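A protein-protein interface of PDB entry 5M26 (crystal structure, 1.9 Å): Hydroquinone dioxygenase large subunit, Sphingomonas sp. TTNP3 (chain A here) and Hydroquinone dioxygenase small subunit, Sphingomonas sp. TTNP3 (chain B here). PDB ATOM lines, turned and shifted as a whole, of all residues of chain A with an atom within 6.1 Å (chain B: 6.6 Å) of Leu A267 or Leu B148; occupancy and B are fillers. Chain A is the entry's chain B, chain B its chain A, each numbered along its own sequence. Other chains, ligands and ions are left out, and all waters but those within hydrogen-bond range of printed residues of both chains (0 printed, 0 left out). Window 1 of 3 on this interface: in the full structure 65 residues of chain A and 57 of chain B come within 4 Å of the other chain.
Leu A267 touches two residues of chain B. Printed residues of chain B within 4 Å of Gly A294: Val B34. Printed residues of chain B within 4 Å of Asp A295: Ser B32. Printed residues of chain B within 4 Å of Ile A296: Ser B32 (2.8 Å), Val B34 (3.9 Å) and Val B49 (3.6 Å). Of the printed residues of chain A, Ser B32 touches Asp A295 and Ile A296. Of the printed residues of chain A, Leu B148 touches Leu A267 (3.3 Å). The nearest residue of chain B that does not touch Leu A267 is Met B80 (4.4 Å). The nearest printed residue of chain B that does not touch Asp A295 is Val B34 (4.9 Å).
The backbone NH (N) of Val B34 is in hydrogen-bond range of the backbone carbonyl oxygen (O) of Gly A294 (2.9 Å). The backbone carbonyl oxygen (O) of Ser B32 sits at hydrogen-bond distance from the backbone NH (N) of Ile A296 (2.8 Å).
The backbone carbonyl oxygen (O) of Ile B57 lies within hydrogen-bond range of the backbone NH (N) of Val B49 (2.8 Å). The backbone carbonyl oxygen (O) of Trp A265 is in hydrogen-bond range of the backbone NH (N) of Trp A318 (2.8 Å). N of Leu B148 sits at hydrogen-bond distance from O of Leu B78. N of Gly A294 sits at hydrogen-bond distance from O of Gln A268. N of Gln A268 is in hydrogen-bond range of O of Asp A295, 2.9 Å away. N of Gln B150 sits at hydrogen-bond distance from O of Phe B76 (2.9 Å).
Hydrophobic or aromatic side chains of chain B that line the printed part of chain A: Val B34, Val B49, Ile B57 and Leu B148. Along chain B the printed residues that touch a printed residue of chain A span positions 32 to 150. Hydrophobic or aromatic side chains of chain A within 4 Å of the printed part of chain B: Phe A245, Trp A265, Leu A267, Ile A296 and Trp A318.
Among the printed residues, pairs that only touch across the chains: Phe A245 with Ile B57, Phe A245 with Gln B150, Trp A265 with Val B49, Leu A267 with Val B34, Leu A267 with Leu B148, Asp A295 with Ser B32, Ile A296 with Val B34, Ile A296 with Val B49 and Trp A318 with Ile B57.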
ATOM      1  N   PHE A 245      11.124  29.367 -15.723  1.00  0.00           N
ATOM      2  CA  PHE A 245      10.284  28.222 -15.377  1.00  0.00           C
ATOM      3  C   PHE A 245       9.100  28.732 -14.537  1.00  0.00           C
ATOM      4  O   PHE A 245       9.309  29.241 -13.429  1.00  0.00           O
ATOM      5  CB  PHE A 245      11.093  27.196 -14.590  1.00  0.00           C
ATOM      6  CG  PHE A 245      11.715  26.108 -15.452  1.00  0.00           C
ATOM      7  CD1 PHE A 245      12.024  26.334 -16.801  1.00  0.00           C
ATOM      8  CD2 PHE A 245      11.989  24.855 -14.905  1.00  0.00           C
ATOM      9  CE1 PHE A 245      12.583  25.308 -17.588  1.00  0.00           C
ATOM     10  CE2 PHE A 245      12.549  23.833 -15.685  1.00  0.00           C
ATOM     11  CZ  PHE A 245      12.857  24.071 -17.019  1.00  0.00           C
ATOM     12  N   TRP A 265       6.356  27.110 -24.178  1.00  0.00           N
ATOM     13  CA  TRP A 265       6.346  25.651 -24.079  1.00  0.00           C
ATOM     14  C   TRP A 265       5.607  25.165 -22.832  1.00  0.00           C
ATOM     15  O   TRP A 265       5.639  25.813 -21.776  1.00  0.00           O
ATOM     16  CB  TRP A 265       7.772  25.105 -24.052  1.00  0.00           C
ATOM     17  CG  TRP A 265       8.556  25.281 -25.303  1.00  0.00           C
ATOM     18  CD1 TRP A 265       9.091  26.455 -25.801  1.00  0.00           C
ATOM     19  CD2 TRP A 265       8.921  24.246 -26.236  1.00  0.00           C
ATOM     20  NE1 TRP A 265       9.761  26.196 -26.977  1.00  0.00           N
ATOM     21  CE2 TRP A 265       9.664  24.859 -27.276  1.00  0.00           C
ATOM     22  CE3 TRP A 265       8.654  22.876 -26.315  1.00  0.00           C
ATOM     23  CZ2 TRP A 265      10.198  24.130 -28.354  1.00  0.00           C
ATOM     24  CZ3 TRP A 265       9.180  22.130 -27.402  1.00  0.00           C
ATOM     25  CH2 TRP A 265       9.935  22.777 -28.410  1.00  0.00           C
ATOM     26  N   PHE A 266       4.963  24.013 -22.967  1.00  0.00           N
ATOM     27  CA  PHE A 266       4.283  23.349 -21.866  1.00  0.00           C
ATOM     28  C   PHE A 266       4.911  21.997 -21.600  1.00  0.00           C
ATOM     29  O   PHE A 266       4.944  21.130 -22.500  1.00  0.00           O
ATOM     30  CB  PHE A 266       2.828  23.080 -22.263  1.00  0.00           C
ATOM     31  CG  PHE A 266       1.994  24.302 -22.435  1.00  0.00           C
ATOM     32  CD1 PHE A 266       2.224  25.447 -21.671  1.00  0.00           C
ATOM     33  CD2 PHE A 266       0.925  24.300 -23.343  1.00  0.00           C
ATOM     34  CE1 PHE A 266       1.424  26.568 -21.822  1.00  0.00           C
ATOM     35  CE2 PHE A 266       0.127  25.419 -23.489  1.00  0.00           C
ATOM     36  CZ  PHE A 266       0.385  26.566 -22.718  1.00  0.00           C
ATOM     37  N   LEU A 267       5.354  21.782 -20.367  1.00  0.00           N
ATOM     38  CA  LEU A 267       5.760  20.450 -19.947  1.00  0.00           C
ATOM     39  C   LEU A 267       4.783  19.985 -18.879  1.00  0.00           C
ATOM     40  O   LEU A 267       4.651  20.618 -17.827  1.00  0.00           O
ATOM     41  CB  LEU A 267       7.227  20.411 -19.467  1.00  0.00           C
ATOM     42  CG  LEU A 267       7.615  19.157 -18.644  1.00  0.00           C
ATOM     43  CD1 LEU A 267       7.663  17.836 -19.432  1.00  0.00           C
ATOM     44  CD2 LEU A 267       8.944  19.383 -17.949  1.00  0.00           C
ATOM     45  N   GLN A 268       4.077  18.888 -19.171  1.00  0.00           N
ATOM     46  CA  GLN A 268       3.097  18.332 -18.257  1.00  0.00           C
ATOM     47  C   GLN A 268       3.817  17.515 -17.206  1.00  0.00           C
ATOM     48  O   GLN A 268       4.532  16.544 -17.544  1.00  0.00           O
ATOM     49  CB  GLN A 268       2.080  17.429 -19.011  1.00  0.00           C
ATOM     50  CG  GLN A 268       0.857  17.064 -18.176  1.00  0.00           C
ATOM     51  CD  GLN A 268      -0.026  18.279 -17.940  1.00  0.00           C
ATOM     52  OE1 GLN A 268      -0.117  19.171 -18.798  1.00  0.00           O
ATOM     53  NE2 GLN A 268      -0.622  18.356 -16.777  1.00  0.00           N
ATOM     54  N   LEU A 269       3.616  17.875 -15.934  1.00  0.00           N
ATOM     55  CA  LEU A 269       4.378  17.286 -14.842  1.00  0.00           C
ATOM     56  C   LEU A 269       3.588  16.182 -14.128  1.00  0.00           C
ATOM     57  O   LEU A 269       4.169  15.198 -13.678  1.00  0.00           O
ATOM     58  CB  LEU A 269       4.814  18.393 -13.840  1.00  0.00           C
ATOM     59  CG  LEU A 269       5.742  19.499 -14.331  1.00  0.00           C
ATOM     60  CD1 LEU A 269       5.917  20.539 -13.227  1.00  0.00           C
ATOM     61  CD2 LEU A 269       7.098  18.979 -14.816  1.00  0.00           C
ATOM     62  N   ALA A 293       1.787  13.000 -18.291  1.00  0.00           N
ATOM     63  CA  ALA A 293       3.004  13.279 -17.521  1.00  0.00           C
ATOM     64  C   ALA A 293       4.272  13.015 -18.355  1.00  0.00           C
ATOM     65  O   ALA A 293       4.407  11.962 -18.986  1.00  0.00           O
ATOM     66  CB  ALA A 293       3.008  12.461 -16.227  1.00  0.00           C
ATOM     67  N   GLY A 294       5.174  13.996 -18.379  1.00  0.00           N
ATOM     68  CA  GLY A 294       6.406  13.935 -19.190  1.00  0.00           C
ATOM     69  C   GLY A 294       6.269  14.505 -20.598  1.00  0.00           C
ATOM     70  O   GLY A 294       7.282  14.749 -21.281  1.00  0.00           O
ATOM     71  N   ASP A 295       5.030  14.737 -21.054  1.00  0.00           N
ATOM     72  CA  ASP A 295       4.815  15.276 -22.416  1.00  0.00           C
ATOM     73  C   ASP A 295       5.196  16.749 -22.495  1.00  0.00           C
ATOM     74  O   ASP A 295       4.726  17.574 -21.702  1.00  0.00           O
ATOM     75  CB  ASP A 295       3.378  15.107 -22.911  1.00  0.00           C
ATOM     76  CG  ASP A 295       3.026  13.651 -23.255  1.00  0.00           C
ATOM     77  OD1 ASP A 295       3.965  12.821 -23.422  1.00  0.00           O
ATOM     78  OD2 ASP A 295       1.798  13.345 -23.384  1.00  0.00           O
ATOM     79  N   ILE A 296       6.009  17.085 -23.486  1.00  0.00           N
ATOM     80  CA  ILE A 296       6.387  18.484 -23.669  1.00  0.00           C
ATOM     81  C   ILE A 296       6.002  18.906 -25.067  1.00  0.00           C
ATOM     82  O   ILE A 296       6.173  18.122 -26.026  1.00  0.00           O
ATOM     83  CB  ILE A 296       7.882  18.765 -23.337  1.00  0.00           C
ATOM     84  CG1 ILE A 296       8.207  20.248 -23.467  1.00  0.00           C
ATOM     85  CG2 ILE A 296       8.854  17.983 -24.220  1.00  0.00           C
ATOM     86  CD1 ILE A 296       9.639  20.550 -23.097  1.00  0.00           C
ATOM     87  N   CYS A 297       5.452  20.110 -25.191  1.00  0.00           N
ATOM     88  CA  CYS A 297       5.135  20.639 -26.505  1.00  0.00           C
ATOM     89  C   CYS A 297       5.274  22.132 -26.538  1.00  0.00           C
ATOM     90  O   CYS A 297       5.427  22.770 -25.491  1.00  0.00           O
ATOM     91  CB  CYS A 297       3.734  20.230 -26.948  1.00  0.00           C
ATOM     92  SG  CYS A 297       2.444  20.883 -25.868  1.00  0.00           S
ATOM     93  N   MET A 314      -0.217  19.298 -12.389  1.00  0.00           N
ATOM     94  CA  MET A 314       0.978  20.112 -12.319  1.00  0.00           C
ATOM     95  C   MET A 314       1.497  20.364 -13.730  1.00  0.00           C
ATOM     96  O   MET A 314       1.752  19.442 -14.508  1.00  0.00           O
ATOM     97  CB  MET A 314       2.033  19.408 -11.483  1.00  0.00           C
ATOM     98  CG  MET A 314       1.589  19.185 -10.049  1.00  0.00           C
ATOM     99  SD  MET A 314       2.936  18.481  -9.082  1.00  0.00           S
ATOM    100  CE  MET A 314       2.066  17.996  -7.574  1.00  0.00           C
ATOM    101  N   LEU A 315       1.627  21.625 -14.079  1.00  0.00           N
ATOM    102  CA  LEU A 315       2.077  22.004 -15.431  1.00  0.00           C
ATOM    103  C   LEU A 315       3.258  22.946 -15.286  1.00  0.00           C
ATOM    104  O   LEU A 315       3.226  23.834 -14.437  1.00  0.00           O
ATOM    105  CB  LEU A 315       0.955  22.722 -16.165  1.00  0.00           C
ATOM    106  CG  LEU A 315       1.322  23.406 -17.486  1.00  0.00           C
ATOM    107  CD1 LEU A 315       1.599  22.382 -18.593  1.00  0.00           C
ATOM    108  CD2 LEU A 315       0.181  24.350 -17.842  1.00  0.00           C
ATOM    109  N   LEU A 316       4.311  22.737 -16.084  1.00  0.00           N
ATOM    110  CA  LEU A 316       5.391  23.704 -16.183  1.00  0.00           C
ATOM    111  C   LEU A 316       5.144  24.546 -17.431  1.00  0.00           C
ATOM    112  O   LEU A 316       5.095  24.006 -18.545  1.00  0.00           O
ATOM    113  CB  LEU A 316       6.749  23.010 -16.313  1.00  0.00           C
ATOM    114  CG  LEU A 316       7.883  23.946 -16.771  1.00  0.00           C
ATOM    115  CD1 LEU A 316       8.196  24.995 -15.701  1.00  0.00           C
ATOM    116  CD2 LEU A 316       9.148  23.162 -17.113  1.00  0.00           C
ATOM    117  N   VAL A 317       4.969  25.850 -17.262  1.00  0.00           N
ATOM    118  CA  VAL A 317       4.913  26.742 -18.408  1.00  0.00           C
ATOM    119  C   VAL A 317       6.316  27.354 -18.516  1.00  0.00           C
ATOM    120  O   VAL A 317       6.841  27.913 -17.532  1.00  0.00           O
ATOM    121  CB  VAL A 317       3.827  27.836 -18.250  1.00  0.00           C
ATOM    122  CG1 VAL A 317       3.887  28.854 -19.390  1.00  0.00           C
ATOM    123  CG2 VAL A 317       2.448  27.192 -18.206  1.00  0.00           C
ATOM    124  N   TRP A 318       6.915  27.262 -19.703  1.00  0.00           N
ATOM    125  CA  TRP A 318       8.267  27.766 -19.912  1.00  0.00           C
ATOM    126  C   TRP A 318       8.284  28.935 -20.873  1.00  0.00           C
ATOM    127  O   TRP A 318       7.896  28.797 -22.044  1.00  0.00           O
ATOM    128  CB  TRP A 318       9.186  26.635 -20.393  1.00  0.00           C
ATOM    129  CG  TRP A 318      10.592  27.075 -20.681  1.00  0.00           C
ATOM    130  CD1 TRP A 318      11.383  27.887 -19.904  1.00  0.00           C
ATOM    131  CD2 TRP A 318      11.373  26.735 -21.825  1.00  0.00           C
ATOM    132  NE1 TRP A 318      12.619  28.067 -20.500  1.00  0.00           N
ATOM    133  CE2 TRP A 318      12.643  27.364 -21.676  1.00  0.00           C
ATOM    134  CE3 TRP A 318      11.138  25.954 -22.966  1.00  0.00           C
ATOM    135  CZ2 TRP A 318      13.652  27.242 -22.630  1.00  0.00           C
ATOM    136  CZ3 TRP A 318      12.142  25.842 -23.906  1.00  0.00           C
ATOM    137  CH2 TRP A 318      13.377  26.472 -23.735  1.00  0.00           C
ATOM    138  N   SER B  32       7.147  15.889 -27.758  1.00  0.00           N
ATOM    139  CA  SER B  32       7.899  14.704 -27.339  1.00  0.00           C
ATOM    140  C   SER B  32       7.527  14.328 -25.896  1.00  0.00           C
ATOM    141  O   SER B  32       6.774  15.055 -25.241  1.00  0.00           O
ATOM    142  CB  SER B  32       9.408  14.919 -27.505  1.00  0.00           C
ATOM    143  OG  SER B  32       9.907  15.918 -26.607  1.00  0.00           O
ATOM    144  N   VAL B  34       9.580  13.462 -22.392  1.00  0.00           N
ATOM    145  CA  VAL B  34      10.926  13.523 -21.823  1.00  0.00           C
ATOM    146  C   VAL B  34      11.402  12.202 -21.246  1.00  0.00           C
ATOM    147  O   VAL B  34      12.610  11.962 -21.194  1.00  0.00           O
ATOM    148  CB  VAL B  34      11.071  14.671 -20.774  1.00  0.00           C
ATOM    149  CG1 VAL B  34      10.538  15.968 -21.367  1.00  0.00           C
ATOM    150  CG2 VAL B  34      10.364  14.359 -19.455  1.00  0.00           C
ATOM    151  N   VAL B  49      14.742  19.011 -25.488  1.00  0.00           N
ATOM    152  CA  VAL B  49      13.304  18.704 -25.644  1.00  0.00           C
ATOM    153  C   VAL B  49      12.480  20.000 -25.786  1.00  0.00           C
ATOM    154  O   VAL B  49      11.337  19.988 -26.243  1.00  0.00           O
ATOM    155  CB  VAL B  49      12.747  17.777 -24.520  1.00  0.00           C
ATOM    156  CG1 VAL B  49      13.383  16.379 -24.585  1.00  0.00           C
ATOM    157  CG2 VAL B  49      12.966  18.373 -23.132  1.00  0.00           C
ATOM    158  N   ILE B  57      15.395  23.361 -22.731  1.00  0.00           N
ATOM    159  CA  ILE B  57      15.172  22.343 -21.717  1.00  0.00           C
ATOM    160  C   ILE B  57      15.784  21.091 -22.318  1.00  0.00           C
ATOM    161  O   ILE B  57      15.485  20.737 -23.469  1.00  0.00           O
ATOM    162  CB  ILE B  57      13.688  22.126 -21.436  1.00  0.00           C
ATOM    163  CG1 ILE B  57      13.102  23.425 -20.844  1.00  0.00           C
ATOM    164  CG2 ILE B  57      13.510  20.961 -20.465  1.00  0.00           C
ATOM    165  CD1 ILE B  57      11.598  23.364 -20.631  1.00  0.00           C
ATOM    166  N   GLU B  58      16.677  20.473 -21.558  1.00  0.00           N
ATOM    167  CA  GLU B  58      17.292  19.205 -21.969  1.00  0.00           C
ATOM    168  C   GLU B  58      16.796  18.055 -21.105  1.00  0.00           C
ATOM    169  O   GLU B  58      16.683  18.201 -19.900  1.00  0.00           O
ATOM    170  CB  GLU B  58      18.807  19.318 -21.810  1.00  0.00           C
ATOM    171  CG  GLU B  58      19.473  20.283 -22.769  1.00  0.00           C
ATOM    172  CD  GLU B  58      20.792  20.811 -22.221  1.00  0.00           C
ATOM    173  OE1 GLU B  58      21.094  20.664 -21.022  1.00  0.00           O
ATOM    174  OE2 GLU B  58      21.544  21.385 -23.000  1.00  0.00           O
ATOM    175  N   SER B  59      16.513  16.910 -21.719  1.00  0.00           N
ATOM    176  CA  SER B  59      16.218  15.690 -20.978  1.00  0.00           C
ATOM    177  C   SER B  59      17.450  14.759 -20.991  1.00  0.00           C
ATOM    178  O   SER B  59      18.142  14.695 -22.009  1.00  0.00           O
ATOM    179  CB  SER B  59      15.035  14.974 -21.638  1.00  0.00           C
ATOM    180  OG  SER B  59      14.654  13.856 -20.866  1.00  0.00           O
ATOM    181  N   ALA B  60      17.700  14.037 -19.889  1.00  0.00           N
ATOM    182  CA  ALA B  60      18.848  13.107 -19.782  1.00  0.00           C
ATOM    183  C   ALA B  60      18.497  11.982 -18.826  1.00  0.00           C
ATOM    184  O   ALA B  60      17.747  12.196 -17.860  1.00  0.00           O
ATOM    185  CB  ALA B  60      20.090  13.830 -19.249  1.00  0.00           C
ATOM    186  N   PHE B  76      19.581  24.903 -13.834  1.00  0.00           N
ATOM    187  CA  PHE B  76      18.794  24.181 -12.843  1.00  0.00           C
ATOM    188  C   PHE B  76      18.578  22.787 -13.335  1.00  0.00           C
ATOM    189  O   PHE B  76      18.499  22.581 -14.538  1.00  0.00           O
ATOM    190  CB  PHE B  76      17.450  24.897 -12.586  1.00  0.00           C
ATOM    191  CG  PHE B  76      17.658  26.299 -12.096  1.00  0.00           C
ATOM    192  CD1 PHE B  76      17.886  26.527 -10.742  1.00  0.00           C
ATOM    193  CD2 PHE B  76      17.784  27.364 -13.004  1.00  0.00           C
ATOM    194  CE1 PHE B  76      18.155  27.816 -10.271  1.00  0.00           C
ATOM    195  CE2 PHE B  76      18.066  28.656 -12.544  1.00  0.00           C
ATOM    196  CZ  PHE B  76      18.254  28.876 -11.178  1.00  0.00           C
ATOM    197  N   VAL B  77      18.524  21.840 -12.403  1.00  0.00           N
ATOM    198  CA  VAL B  77      18.181  20.465 -12.746  1.00  0.00           C
ATOM    199  C   VAL B  77      16.954  20.071 -11.935  1.00  0.00           C
ATOM    200  O   VAL B  77      16.867  20.359 -10.751  1.00  0.00           O
ATOM    201  CB  VAL B  77      19.376  19.483 -12.564  1.00  0.00           C
ATOM    202  CG1 VAL B  77      19.951  19.542 -11.149  1.00  0.00           C
ATOM    203  CG2 VAL B  77      18.935  18.049 -12.870  1.00  0.00           C
ATOM    204  N   LEU B  78      15.995  19.436 -12.591  1.00  0.00           N
ATOM    205  CA  LEU B  78      14.803  18.928 -11.941  1.00  0.00           C
ATOM    206  C   LEU B  78      14.804  17.424 -12.157  1.00  0.00           C
ATOM    207  O   LEU B  78      14.799  16.976 -13.303  1.00  0.00           O
ATOM    208  CB  LEU B  78      13.560  19.518 -12.618  1.00  0.00           C
ATOM    209  CG  LEU B  78      12.178  18.936 -12.291  1.00  0.00           C
ATOM    210  CD1 LEU B  78      11.891  19.010 -10.804  1.00  0.00           C
ATOM    211  CD2 LEU B  78      11.055  19.618 -13.086  1.00  0.00           C
ATOM    212  N   ALA B  79      14.804  16.654 -11.066  1.00  0.00           N
ATOM    213  CA  ALA B  79      14.736  15.198 -11.152  1.00  0.00           C
ATOM    214  C   ALA B  79      13.301  14.833 -11.457  1.00  0.00           C
ATOM    215  O   ALA B  79      12.388  15.420 -10.901  1.00  0.00           O
ATOM    216  CB  ALA B  79      15.168  14.572  -9.839  1.00  0.00           C
ATOM    217  N   MET B  80      13.103  13.876 -12.354  1.00  0.00           N
ATOM    218  CA  MET B  80      11.753  13.527 -12.792  1.00  0.00           C
ATOM    219  C   MET B  80      11.331  12.129 -12.380  1.00  0.00           C
ATOM    220  O   MET B  80      10.150  11.805 -12.445  1.00  0.00           O
ATOM    221  CB  MET B  80      11.622  13.659 -14.308  1.00  0.00           C
ATOM    222  CG  MET B  80      11.654  15.084 -14.834  1.00  0.00           C
ATOM    223  SD  MET B  80      10.157  15.993 -14.383  1.00  0.00           S
ATOM    224  CE  MET B  80       9.074  15.533 -15.733  1.00  0.00           C
ATOM    225  N   ALA B 146      15.508   9.822 -14.495  1.00  0.00           N
ATOM    226  CA  ALA B 146      15.285  10.849 -15.510  1.00  0.00           C
ATOM    227  C   ALA B 146      15.500  12.240 -14.905  1.00  0.00           C
ATOM    228  O   ALA B 146      15.160  12.468 -13.742  1.00  0.00           O
ATOM    229  CB  ALA B 146      13.878  10.739 -16.076  1.00  0.00           C
ATOM    230  N   MET B 147      16.065  13.162 -15.674  1.00  0.00           N
ATOM    231  CA  MET B 147      16.242  14.533 -15.172  1.00  0.00           C
ATOM    232  C   MET B 147      16.145  15.543 -16.302  1.00  0.00           C
ATOM    233  O   MET B 147      16.293  15.192 -17.484  1.00  0.00           O
ATOM    234  CB  MET B 147      17.562  14.711 -14.404  1.00  0.00           C
ATOM    235  CG  MET B 147      18.815  14.605 -15.248  1.00  0.00           C
ATOM    236  SD  MET B 147      20.258  14.547 -14.146  1.00  0.00           S
ATOM    237  CE  MET B 147      21.379  13.880 -15.338  1.00  0.00           C
ATOM    238  N   LEU B 148      15.885  16.794 -15.931  1.00  0.00           N
ATOM    239  CA  LEU B 148      15.683  17.840 -16.906  1.00  0.00           C
ATOM    240  C   LEU B 148      16.583  18.975 -16.535  1.00  0.00           C
ATOM    241  O   LEU B 148      16.739  19.257 -15.345  1.00  0.00           O
ATOM    242  CB  LEU B 148      14.241  18.359 -16.846  1.00  0.00           C
ATOM    243  CG  LEU B 148      13.163  17.397 -17.329  1.00  0.00           C
ATOM    244  CD1 LEU B 148      11.842  18.073 -17.052  1.00  0.00           C
ATOM    245  CD2 LEU B 148      13.340  17.158 -18.826  1.00  0.00           C
ATOM    246  N   PHE B 149      17.119  19.660 -17.539  1.00  0.00           N
ATOM    247  CA  PHE B 149      17.947  20.830 -17.292  1.00  0.00           C
ATOM    248  C   PHE B 149      17.306  22.069 -17.881  1.00  0.00           C
ATOM    249  O   PHE B 149      16.828  22.049 -19.025  1.00  0.00           O
ATOM    250  CB  PHE B 149      19.331  20.658 -17.937  1.00  0.00           C
ATOM    251  CG  PHE B 149      20.199  19.612 -17.295  1.00  0.00           C
ATOM    252  CD1 PHE B 149      20.173  18.302 -17.744  1.00  0.00           C
ATOM    253  CD2 PHE B 149      21.115  19.962 -16.298  1.00  0.00           C
ATOM    254  CE1 PHE B 149      21.010  17.347 -17.190  1.00  0.00           C
ATOM    255  CE2 PHE B 149      21.956  19.009 -15.736  1.00  0.00           C
ATOM    256  CZ  PHE B 149      21.902  17.696 -16.196  1.00  0.00           C
ATOM    257  N   GLN B 150      17.274  23.136 -17.084  1.00  0.00           N
ATOM    258  CA  GLN B 150      16.978  24.459 -17.598  1.00  0.00           C
ATOM    259  C   GLN B 150      18.313  25.138 -17.910  1.00  0.00           C
ATOM    260  O   GLN B 150      19.108  25.463 -16.999  1.00  0.00           O
ATOM    261  CB  GLN B 150      16.153  25.259 -16.568  1.00  0.00           C
ATOM    262  CG  GLN B 150      15.925  26.712 -16.961  1.00  0.00           C
ATOM    263  CD  GLN B 150      15.132  27.467 -15.919  1.00  0.00           C
ATOM    264  OE1 GLN B 150      14.971  26.998 -14.784  1.00  0.00           O
ATOM    265  NE2 GLN B 150      14.627  28.628 -16.296  1.00  0.00           N
